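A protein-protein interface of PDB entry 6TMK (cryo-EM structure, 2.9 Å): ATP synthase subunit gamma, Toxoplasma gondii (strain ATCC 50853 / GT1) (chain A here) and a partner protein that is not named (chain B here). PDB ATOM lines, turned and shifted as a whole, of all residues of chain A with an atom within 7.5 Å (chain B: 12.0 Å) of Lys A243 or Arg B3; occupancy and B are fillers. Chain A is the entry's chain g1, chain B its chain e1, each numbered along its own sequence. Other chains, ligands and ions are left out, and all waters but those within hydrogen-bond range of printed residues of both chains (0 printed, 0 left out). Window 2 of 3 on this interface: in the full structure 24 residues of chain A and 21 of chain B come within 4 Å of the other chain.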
ATOM      1  N   ASP A 185     -19.791  25.668  13.173  1.00  0.00           N
ATOM      2  CA  ASP A 185     -18.864  24.612  13.555  1.00  0.00           C
ATOM      3  C   ASP A 185     -19.601  23.432  14.171  1.00  0.00           C
ATOM      4  O   ASP A 185     -19.252  22.276  13.915  1.00  0.00           O
ATOM      5  CB  ASP A 185     -17.823  25.163  14.525  1.00  0.00           C
ATOM      6  CG  ASP A 185     -16.743  25.965  13.825  1.00  0.00           C
ATOM      7  OD1 ASP A 185     -15.731  26.297  14.476  1.00  0.00           O
ATOM      8  OD2 ASP A 185     -16.906  26.265  12.623  1.00  0.00           O
ATOM      9  N   MET A 188     -21.068  21.482  11.346  1.00  0.00           N
ATOM     10  CA  MET A 188     -20.118  20.731  10.541  1.00  0.00           C
ATOM     11  C   MET A 188     -19.616  19.538  11.337  1.00  0.00           C
ATOM     12  O   MET A 188     -19.398  18.456  10.779  1.00  0.00           O
ATOM     13  CB  MET A 188     -18.968  21.630  10.090  1.00  0.00           C
ATOM     14  CG  MET A 188     -18.119  21.019   8.988  1.00  0.00           C
ATOM     15  SD  MET A 188     -19.012  20.879   7.426  1.00  0.00           S
ATOM     16  CE  MET A 188     -18.961  22.569   6.844  1.00  0.00           C
ATOM     17  N   PRO A 218     -21.298  19.071   2.648  1.00  0.00           N
ATOM     18  CA  PRO A 218     -20.152  18.349   2.076  1.00  0.00           C
ATOM     19  C   PRO A 218     -20.549  17.168   1.209  1.00  0.00           C
ATOM     20  O   PRO A 218     -19.886  16.903   0.201  1.00  0.00           O
ATOM     21  CB  PRO A 218     -19.380  17.904   3.323  1.00  0.00           C
ATOM     22  CG  PRO A 218     -19.698  18.938   4.341  1.00  0.00           C
ATOM     23  CD  PRO A 218     -21.125  19.321   4.089  1.00  0.00           C
ATOM     24  N   GLU A 237      -5.544  25.731  -4.512  1.00  0.00           N
ATOM     25  CA  GLU A 237      -6.310  24.798  -5.322  1.00  0.00           C
ATOM     26  C   GLU A 237      -7.700  24.575  -4.730  1.00  0.00           C
ATOM     27  O   GLU A 237      -7.945  24.769  -3.533  1.00  0.00           O
ATOM     28  CB  GLU A 237      -5.570  23.463  -5.431  1.00  0.00           C
ATOM     29  CG  GLU A 237      -6.062  22.550  -6.538  1.00  0.00           C
ATOM     30  CD  GLU A 237      -5.829  21.086  -6.227  1.00  0.00           C
ATOM     31  OE1 GLU A 237      -4.997  20.787  -5.346  1.00  0.00           O
ATOM     32  OE2 GLU A 237      -6.483  20.232  -6.864  1.00  0.00           O
ATOM     33  N   LYS A 238      -8.622  24.178  -5.607  1.00  0.00           N
ATOM     34  CA  LYS A 238     -10.017  24.059  -5.209  1.00  0.00           C
ATOM     35  C   LYS A 238     -10.176  23.032  -4.100  1.00  0.00           C
ATOM     36  O   LYS A 238     -10.908  23.258  -3.132  1.00  0.00           O
ATOM     37  CB  LYS A 238     -10.874  23.684  -6.418  1.00  0.00           C
ATOM     38  CG  LYS A 238     -12.363  23.806  -6.181  1.00  0.00           C
ATOM     39  CD  LYS A 238     -13.154  23.387  -7.404  1.00  0.00           C
ATOM     40  CE  LYS A 238     -13.139  24.461  -8.477  1.00  0.00           C
ATOM     41  NZ  LYS A 238     -13.997  24.094  -9.639  1.00  0.00           N
ATOM     42  N   THR A 239      -9.481  21.896  -4.214  1.00  0.00           N
ATOM     43  CA  THR A 239      -9.654  20.826  -3.239  1.00  0.00           C
ATOM     44  C   THR A 239      -9.142  21.229  -1.865  1.00  0.00           C
ATOM     45  O   THR A 239      -9.634  20.722  -0.851  1.00  0.00           O
ATOM     46  CB  THR A 239      -8.937  19.564  -3.716  1.00  0.00           C
ATOM     47  OG1 THR A 239      -7.539  19.836  -3.874  1.00  0.00           O
ATOM     48  CG2 THR A 239      -9.512  19.095  -5.038  1.00  0.00           C
ATOM     49  N   ASP A 240      -8.164  22.131  -1.805  1.00  0.00           N
ATOM     50  CA  ASP A 240      -7.594  22.526  -0.526  1.00  0.00           C
ATOM     51  C   ASP A 240      -8.323  23.713   0.081  1.00  0.00           C
ATOM     52  O   ASP A 240      -8.334  23.865   1.308  1.00  0.00           O
ATOM     53  CB  ASP A 240      -6.106  22.864  -0.675  1.00  0.00           C
ATOM     54  CG  ASP A 240      -5.852  23.987  -1.660  1.00  0.00           C
ATOM     55  OD1 ASP A 240      -5.011  23.805  -2.564  1.00  0.00           O
ATOM     56  OD2 ASP A 240      -6.468  25.062  -1.514  1.00  0.00           O
ATOM     57  N   VAL A 241      -8.934  24.558  -0.754  1.00  0.00           N
ATOM     58  CA  VAL A 241      -9.624  25.748  -0.266  1.00  0.00           C
ATOM     59  C   VAL A 241     -11.124  25.538  -0.096  1.00  0.00           C
ATOM     60  O   VAL A 241     -11.785  26.378   0.537  1.00  0.00           O
ATOM     61  CB  VAL A 241      -9.371  26.947  -1.206  1.00  0.00           C
ATOM     62  CG1 VAL A 241     -10.169  26.798  -2.488  1.00  0.00           C
ATOM     63  CG2 VAL A 241      -9.703  28.256  -0.512  1.00  0.00           C
ATOM     64  N   TRP A 242     -11.682  24.449  -0.629  1.00  0.00           N
ATOM     65  CA  TRP A 242     -13.122  24.234  -0.541  1.00  0.00           C
ATOM     66  C   TRP A 242     -13.577  24.050   0.900  1.00  0.00           C
ATOM     67  O   TRP A 242     -14.612  24.588   1.305  1.00  0.00           O
ATOM     68  CB  TRP A 242     -13.523  23.020  -1.374  1.00  0.00           C
ATOM     69  CG  TRP A 242     -14.995  22.828  -1.442  1.00  0.00           C
ATOM     70  CD1 TRP A 242     -15.719  21.825  -0.873  1.00  0.00           C
ATOM     71  CD2 TRP A 242     -15.935  23.670  -2.118  1.00  0.00           C
ATOM     72  NE1 TRP A 242     -17.053  21.987  -1.155  1.00  0.00           N
ATOM     73  CE2 TRP A 242     -17.210  23.114  -1.918  1.00  0.00           C
ATOM     74  CE3 TRP A 242     -15.819  24.839  -2.874  1.00  0.00           C
ATOM     75  CZ2 TRP A 242     -18.364  23.685  -2.446  1.00  0.00           C
ATOM     76  CZ3 TRP A 242     -16.964  25.406  -3.397  1.00  0.00           C
ATOM     77  CH2 TRP A 242     -18.220  24.829  -3.181  1.00  0.00           C
ATOM     78  N   LYS A 243     -12.831  23.270   1.683  1.00  0.00           N
ATOM     79  CA  LYS A 243     -13.243  22.997   3.055  1.00  0.00           C
ATOM     80  C   LYS A 243     -13.190  24.245   3.922  1.00  0.00           C
ATOM     81  O   LYS A 243     -13.967  24.367   4.875  1.00  0.00           O
ATOM     82  CB  LYS A 243     -12.364  21.904   3.653  1.00  0.00           C
ATOM     83  CG  LYS A 243     -12.635  20.528   3.090  1.00  0.00           C
ATOM     84  CD  LYS A 243     -11.747  19.490   3.740  1.00  0.00           C
ATOM     85  CE  LYS A 243     -11.718  18.206   2.935  1.00  0.00           C
ATOM     86  NZ  LYS A 243     -10.540  17.363   3.280  1.00  0.00           N
ATOM     87  N   ASP A 244     -12.290  25.177   3.613  1.00  0.00           N
ATOM     88  CA  ASP A 244     -12.217  26.417   4.375  1.00  0.00           C
ATOM     89  C   ASP A 244     -13.224  27.439   3.869  1.00  0.00           C
ATOM     90  O   ASP A 244     -13.663  28.304   4.634  1.00  0.00           O
ATOM     91  CB  ASP A 244     -10.804  26.992   4.306  1.00  0.00           C
ATOM     92  CG  ASP A 244      -9.778  26.091   4.961  1.00  0.00           C
ATOM     93  OD1 ASP A 244     -10.144  25.354   5.901  1.00  0.00           O
ATOM     94  OD2 ASP A 244      -8.604  26.116   4.535  1.00  0.00           O
ATOM     95  N   LEU A 245     -13.596  27.353   2.592  1.00  0.00           N
ATOM     96  CA  LEU A 245     -14.629  28.228   2.055  1.00  0.00           C
ATOM     97  C   LEU A 245     -16.014  27.812   2.532  1.00  0.00           C
ATOM     98  O   LEU A 245     -16.890  28.664   2.722  1.00  0.00           O
ATOM     99  CB  LEU A 245     -14.566  28.227   0.530  1.00  0.00           C
ATOM    100  CG  LEU A 245     -15.612  29.057  -0.206  1.00  0.00           C
ATOM    101  CD1 LEU A 245     -15.464  30.527   0.132  1.00  0.00           C
ATOM    102  CD2 LEU A 245     -15.480  28.835  -1.696  1.00  0.00           C
ATOM    103  N   GLN A 246     -16.231  26.511   2.730  1.00  0.00           N
ATOM    104  CA  GLN A 246     -17.562  26.027   3.078  1.00  0.00           C
ATOM    105  C   GLN A 246     -17.954  26.449   4.489  1.00  0.00           C
ATOM    106  O   GLN A 246     -19.124  26.754   4.751  1.00  0.00           O
ATOM    107  CB  GLN A 246     -17.600  24.506   2.941  1.00  0.00           C
ATOM    108  CG  GLN A 246     -18.966  23.938   2.649  1.00  0.00           C
ATOM    109  CD  GLN A 246     -18.939  22.440   2.468  1.00  0.00           C
ATOM    110  OE1 GLN A 246     -17.902  21.801   2.642  1.00  0.00           O
ATOM    111  NE2 GLN A 246     -20.080  21.867   2.108  1.00  0.00           N
ATOM    112  N   ASP A 247     -16.991  26.483   5.411  1.00  0.00           N
ATOM    113  CA  ASP A 247     -17.285  26.948   6.762  1.00  0.00           C
ATOM    114  C   ASP A 247     -17.624  28.434   6.767  1.00  0.00           C
ATOM    115  O   ASP A 247     -18.543  28.869   7.471  1.00  0.00           O
ATOM    116  CB  ASP A 247     -16.098  26.668   7.680  1.00  0.00           C
ATOM    117  CG  ASP A 247     -15.589  25.248   7.558  1.00  0.00           C
ATOM    118  OD1 ASP A 247     -16.337  24.390   7.048  1.00  0.00           O
ATOM    119  OD2 ASP A 247     -14.440  24.989   7.972  1.00  0.00           O
ATOM    120  N   PHE A 248     -16.886  29.224   5.987  1.00  0.00           N
ATOM    121  CA  PHE A 248     -17.231  30.629   5.807  1.00  0.00           C
ATOM    122  C   PHE A 248     -18.633  30.779   5.235  1.00  0.00           C
ATOM    123  O   PHE A 248     -19.390  31.664   5.647  1.00  0.00           O
ATOM    124  CB  PHE A 248     -16.205  31.290   4.890  1.00  0.00           C
ATOM    125  CG  PHE A 248     -16.071  32.769   5.089  1.00  0.00           C
ATOM    126  CD1 PHE A 248     -15.548  33.281   6.261  1.00  0.00           C
ATOM    127  CD2 PHE A 248     -16.456  33.648   4.093  1.00  0.00           C
ATOM    128  CE1 PHE A 248     -15.419  34.641   6.439  1.00  0.00           C
ATOM    129  CE2 PHE A 248     -16.330  35.009   4.266  1.00  0.00           C
ATOM    130  CZ  PHE A 248     -15.810  35.505   5.439  1.00  0.00           C
ATOM    131  N   MET B   1      -3.102  23.880   7.785  1.00  0.00           N
ATOM    132  CA  MET B   1      -2.646  23.794   9.203  1.00  0.00           C
ATOM    133  C   MET B   1      -3.799  23.491  10.150  1.00  0.00           C
ATOM    134  O   MET B   1      -3.586  23.285  11.345  1.00  0.00           O
ATOM    135  CB  MET B   1      -1.964  25.093   9.629  1.00  0.00           C
ATOM    136  CG  MET B   1      -1.137  25.759   8.544  1.00  0.00           C
ATOM    137  SD  MET B   1      -0.071  27.057   9.198  1.00  0.00           S
ATOM    138  CE  MET B   1       1.068  26.099  10.196  1.00  0.00           C
ATOM    139  N   TRP B   2      -5.018  23.469   9.624  1.00  0.00           N
ATOM    140  CA  TRP B   2      -6.205  23.355  10.462  1.00  0.00           C
ATOM    141  C   TRP B   2      -6.970  22.068  10.219  1.00  0.00           C
ATOM    142  O   TRP B   2      -7.467  21.464  11.170  1.00  0.00           O
ATOM    143  CB  TRP B   2      -7.143  24.549  10.230  1.00  0.00           C
ATOM    144  CG  TRP B   2      -6.441  25.839  10.366  1.00  0.00           C
ATOM    145  CD1 TRP B   2      -6.159  26.498  11.519  1.00  0.00           C
ATOM    146  CD2 TRP B   2      -5.938  26.652   9.302  1.00  0.00           C
ATOM    147  NE1 TRP B   2      -5.495  27.667  11.245  1.00  0.00           N
ATOM    148  CE2 TRP B   2      -5.350  27.786   9.888  1.00  0.00           C
ATOM    149  CE3 TRP B   2      -5.926  26.528   7.912  1.00  0.00           C
ATOM    150  CZ2 TRP B   2      -4.753  28.791   9.131  1.00  0.00           C
ATOM    151  CZ3 TRP B   2      -5.333  27.525   7.162  1.00  0.00           C
ATOM    152  CH2 TRP B   2      -4.757  28.642   7.773  1.00  0.00           C
ATOM    153  N   ARG B   3      -7.069  21.622   8.967  1.00  0.00           N
ATOM    154  CA  ARG B   3      -7.631  20.309   8.695  1.00  0.00           C
ATOM    155  C   ARG B   3      -6.746  19.193   9.228  1.00  0.00           C
ATOM    156  O   ARG B   3      -7.238  18.084   9.465  1.00  0.00           O
ATOM    157  CB  ARG B   3      -7.834  20.133   7.189  1.00  0.00           C
ATOM    158  CG  ARG B   3      -8.798  21.134   6.573  1.00  0.00           C
ATOM    159  CD  ARG B   3     -10.212  20.595   6.492  1.00  0.00           C
ATOM    160  NE  ARG B   3     -10.916  20.756   7.761  1.00  0.00           N
ATOM    161  CZ  ARG B   3     -11.565  21.858   8.123  1.00  0.00           C
ATOM    162  NH1 ARG B   3     -11.602  22.913   7.320  1.00  0.00           N
ATOM    163  NH2 ARG B   3     -12.175  21.908   9.297  1.00  0.00           N
ATOM    164  N   SER B   4      -5.454  19.463   9.427  1.00  0.00           N
ATOM    165  CA  SER B   4      -4.580  18.515  10.106  1.00  0.00           C
ATOM    166  C   SER B   4      -4.758  18.568  11.618  1.00  0.00           C
ATOM    167  O   SER B   4      -4.816  17.523  12.276  1.00  0.00           O
ATOM    168  CB  SER B   4      -3.125  18.799   9.737  1.00  0.00           C
ATOM    169  OG  SER B   4      -2.612  19.878  10.497  1.00  0.00           O
ATOM    170  N   SER B   5      -4.845  19.769  12.180  1.00  0.00           N
ATOM    171  CA  SER B   5      -5.033  19.953  13.613  1.00  0.00           C
ATOM    172  C   SER B   5      -6.461  19.684  14.070  1.00  0.00           C
ATOM    173  O   SER B   5      -6.734  19.771  15.272  1.00  0.00           O
ATOM    174  CB  SER B   5      -4.621  21.373  14.009  1.00  0.00           C
ATOM    175  OG  SER B   5      -3.304  21.659  13.576  1.00  0.00           O
ATOM    176  N   GLY B   6      -7.372  19.367  13.154  1.00  0.00           N
ATOM    177  CA  GLY B   6      -8.762  19.160  13.505  1.00  0.00           C
ATOM    178  C   GLY B   6      -9.422  20.439  13.969  1.00  0.00           C
ATOM    179  O   GLY B   6     -10.022  20.498  15.045  1.00  0.00           O
ATOM    180  N   VAL B   7      -9.307  21.477  13.145  1.00  0.00           N
ATOM    181  CA  VAL B   7      -9.786  22.812  13.472  1.00  0.00           C
ATOM    182  C   VAL B   7     -10.440  23.401  12.231  1.00  0.00           C
ATOM    183  O   VAL B   7     -10.030  23.124  11.099  1.00  0.00           O
ATOM    184  CB  VAL B   7      -8.652  23.714  13.996  1.00  0.00           C
ATOM    185  CG1 VAL B   7      -9.168  25.103  14.278  1.00  0.00           C
ATOM    186  CG2 VAL B   7      -8.068  23.116  15.257  1.00  0.00           C
ATOM    187  N   SER B   8     -11.464  24.215  12.448  1.00  0.00           N
ATOM    188  CA  SER B   8     -12.198  24.837  11.359  1.00  0.00           C
ATOM    189  C   SER B   8     -11.644  26.216  11.024  1.00  0.00           C
ATOM    190  O   SER B   8     -11.048  26.899  11.865  1.00  0.00           O
ATOM    191  CB  SER B   8     -13.679  24.953  11.716  1.00  0.00           C
ATOM    192  OG  SER B   8     -14.314  25.956  10.943  1.00  0.00           O
ATOM    193  N   PHE B   9     -11.866  26.624   9.773  1.00  0.00           N
ATOM    194  CA  PHE B   9     -11.414  27.936   9.334  1.00  0.00           C
ATOM    195  C   PHE B   9     -12.149  29.040  10.073  1.00  0.00           C
ATOM    196  O   PHE B   9     -11.567  30.093  10.341  1.00  0.00           O
ATOM    197  CB  PHE B   9     -11.604  28.081   7.826  1.00  0.00           C
ATOM    198  CG  PHE B   9     -11.128  29.393   7.280  1.00  0.00           C
ATOM    199  CD1 PHE B   9      -9.779  29.674   7.190  1.00  0.00           C
ATOM    200  CD2 PHE B   9     -12.034  30.340   6.841  1.00  0.00           C
ATOM    201  CE1 PHE B   9      -9.343  30.882   6.685  1.00  0.00           C
ATOM    202  CE2 PHE B   9     -11.604  31.546   6.333  1.00  0.00           C
ATOM    203  CZ  PHE B   9     -10.257  31.816   6.254  1.00  0.00           C
ATOM    204  N   THR B  10     -13.407  28.806  10.445  1.00  0.00           N
ATOM    205  CA  THR B  10     -14.141  29.816  11.196  1.00  0.00           C
ATOM    206  C   THR B  10     -13.557  29.968  12.592  1.00  0.00           C
ATOM    207  O   THR B  10     -13.388  31.089  13.088  1.00  0.00           O
ATOM    208  CB  THR B  10     -15.619  29.439  11.269  1.00  0.00           C
ATOM    209  OG1 THR B  10     -15.751  28.129  11.831  1.00  0.00           O
ATOM    210  CG2 THR B  10     -16.244  29.468   9.884  1.00  0.00           C
ATOM    211  N   ARG B  11     -13.227  28.846  13.232  1.00  0.00           N
ATOM    212  CA  ARG B  11     -12.581  28.891  14.539  1.00  0.00           C
ATOM    213  C   ARG B  11     -11.255  29.635  14.465  1.00  0.00           C
ATOM    214  O   ARG B  11     -10.970  30.508  15.292  1.00  0.00           O
ATOM    215  CB  ARG B  11     -12.365  27.471  15.054  1.00  0.00           C
ATOM    216  CG  ARG B  11     -11.884  27.405  16.483  1.00  0.00           C
ATOM    217  CD  ARG B  11     -11.916  25.984  17.007  1.00  0.00           C
ATOM    218  NE  ARG B  11     -11.341  25.880  18.343  1.00  0.00           N
ATOM    219  CZ  ARG B  11     -11.149  24.734  18.986  1.00  0.00           C
ATOM    220  NH1 ARG B  11     -11.486  23.585  18.419  1.00  0.00           N
ATOM    221  NH2 ARG B  11     -10.617  24.736  20.198  1.00  0.00           N
ATOM    222  N   TYR B  12     -10.420  29.288  13.482  1.00  0.00           N
ATOM    223  CA  TYR B  12      -9.132  29.957  13.335  1.00  0.00           C
ATOM    224  C   TYR B  12      -9.311  31.450  13.078  1.00  0.00           C
ATOM    225  O   TYR B  12      -8.620  32.281  13.683  1.00  0.00           O
ATOM    226  CB  TYR B  12      -8.330  29.288  12.218  1.00  0.00           C
ATOM    227  CG  TYR B  12      -7.392  30.201  11.467  1.00  0.00           C
ATOM    228  CD1 TYR B  12      -6.169  30.567  12.002  1.00  0.00           C
ATOM    229  CD2 TYR B  12      -7.705  30.645  10.192  1.00  0.00           C
ATOM    230  CE1 TYR B  12      -5.305  31.386  11.309  1.00  0.00           C
ATOM    231  CE2 TYR B  12      -6.847  31.460   9.492  1.00  0.00           C
ATOM    232  CZ  TYR B  12      -5.650  31.832  10.055  1.00  0.00           C
ATOM    233  OH  TYR B  12      -4.788  32.644   9.356  1.00  0.00           O
ATOM    234  N   ALA B  13     -10.251  31.813  12.205  1.00  0.00           N
ATOM    235  CA  ALA B  13     -10.458  33.217  11.881  1.00  0.00           C
ATOM    236  C   ALA B  13     -10.919  33.991  13.104  1.00  0.00           C
ATOM    237  O   ALA B  13     -10.457  35.110  13.350  1.00  0.00           O
ATOM    238  CB  ALA B  13     -11.470  33.345  10.746  1.00  0.00           C
ATOM    239  N   GLU B  15     -10.443  33.168  16.363  1.00  0.00           N
ATOM    240  CA  GLU B  15      -9.378  33.205  17.354  1.00  0.00           C
ATOM    241  C   GLU B  15      -8.231  34.118  16.936  1.00  0.00           C
ATOM    242  O   GLU B  15      -7.460  34.553  17.797  1.00  0.00           O
ATOM    243  CB  GLU B  15      -8.875  31.788  17.612  1.00  0.00           C
ATOM    244  CG  GLU B  15      -9.903  30.926  18.327  1.00  0.00           C
ATOM    245  CD  GLU B  15      -9.332  29.622  18.846  1.00  0.00           C
ATOM    246  OE1 GLU B  15      -8.133  29.586  19.183  1.00  0.00           O
ATOM    247  OE2 GLU B  15     -10.088  28.630  18.919  1.00  0.00           O
ATOM    248  N   PHE B  63     -15.741  27.217  21.428  1.00  0.00           N
ATOM    249  CA  PHE B  63     -15.373  26.345  20.322  1.00  0.00           C
ATOM    250  C   PHE B  63     -14.838  25.015  20.826  1.00  0.00           C
ATOM    251  O   PHE B  63     -14.994  23.991  20.152  1.00  0.00           O
ATOM    252  CB  PHE B  63     -14.332  27.027  19.437  1.00  0.00           C
ATOM    253  CG  PHE B  63     -14.917  27.959  18.422  1.00  0.00           C
ATOM    254  CD1 PHE B  63     -14.574  29.296  18.418  1.00  0.00           C
ATOM    255  CD2 PHE B  63     -15.792  27.494  17.459  1.00  0.00           C
ATOM    256  CE1 PHE B  63     -15.103  30.154  17.481  1.00  0.00           C
ATOM    257  CE2 PHE B  63     -16.324  28.349  16.520  1.00  0.00           C
ATOM    258  CZ  PHE B  63     -15.981  29.681  16.532  1.00  0.00           C
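OG of Ser B8 sits at hydrogen-bond distance from OD2 of Asp A185 (3.1 Å).
The side-chain carboxylate of Asp A244 is in salt-bridge range of the guanidinium group of Arg B3 (3.2 Å).
The side-chain hydroxyl of Thr B10 lies close to the side-chain carboxylate of Asp A185.
The side-chain carboxylate (OD2) of Asp A247 is in salt-bridge range of the guanidinium group (NH1) of Arg B3, 3.6 Å away.
The side-chain carboxylate of Asp A247 sits at hydrogen-bond distance from the side-chain hydroxyl of Ser B8.
The side-chain hydroxyl (OG) of Ser B8 lies within hydrogen-bond range of the side-chain hydroxyl (OG1) of Thr B10 (2.8 Å).
The guanidinium group (NE) of Arg B11 lies within salt-bridge range of the side-chain carboxylate (OE2) of Glu B15 (3.1 Å).
The guanidinium group (NH2) of Arg B3 sits at hydrogen-bond distance from the backbone carbonyl oxygen (O) of Val B7, at 3.1 Å.
Arg B11 touches Asp A185 (CB to OD1, 3.6 Å).
Phe B63 touches Asp A185.
CD of Lys A243 touches CD of Arg B3 (3.3 Å).
Phe B9 touches Asp A244.
Asp A247 touches Phe B9 (OD2 to N, 3.5 Å).
Thr B10 touches Asp A247.
N of Phe A248 touches CG2 of Thr B10 (3.96 Å).
Printed residues of chain B within 4 Å of Asp A185: Ser B8, Thr B10, Arg B11 and Phe B63.
No residue of chain B comes within 4 Å of Val A241.
No residue of chain B comes within 4 Å of Trp A242.
Lys A243 touches just one residue of chain B: Arg B3 (3.3 Å).
Of the printed residues of chain B, Asp A244 touches Arg B3 (3.2 Å) and Phe B9 (3.4 Å).
Asp A247 touches just these residues of chain B: Arg B3 (3.6 Å), Ser B8 (3.1 Å), Phe B9 (3.5 Å) and Thr B10 (3.4 Å).
Of the printed residues of chain B, Phe A248 touches Thr B10 (3.96 Å).
Printed residues of chain A within 4 Å of Arg B3: Lys A243, Asp A244 and Asp A247.
Ser B4 touches none of the printed residues of chain A.
Printed residues of chain A within 4 Å of Phe B9: Asp A244 and Asp A247.
Printed residues of chain A within 4 Å of Arg B11: Asp A185.
The nearest residue of chain B that does not touch Lys A243 is Phe B9 (5.3 Å).
Of the 15 printed residues of chain A, 5 touch a printed residue of chain B.
Printed residues of chain A that touch a printed residue of chain B: Asp A185, Lys A243, Asp A244, Asp A247 and Phe A248.
Of the 15 printed residues of chain B, 6 touch a printed residue of chain A.
Printed residues of chain B that touch a printed residue of chain A: Arg B3, Ser B8, Phe B9, Thr B10, Arg B11 and Phe B63.
Hydrophobic or aromatic side chains of chain B within 4 Å of the printed part of chain A: Phe B9 and Phe B63.
Among the printed residues, Asp or Glu carboxylates within 4 Å of a Lys or Arg side-chain nitrogen of the other chain: Asp A244 with Arg B3 and Asp A247 with Arg B3.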
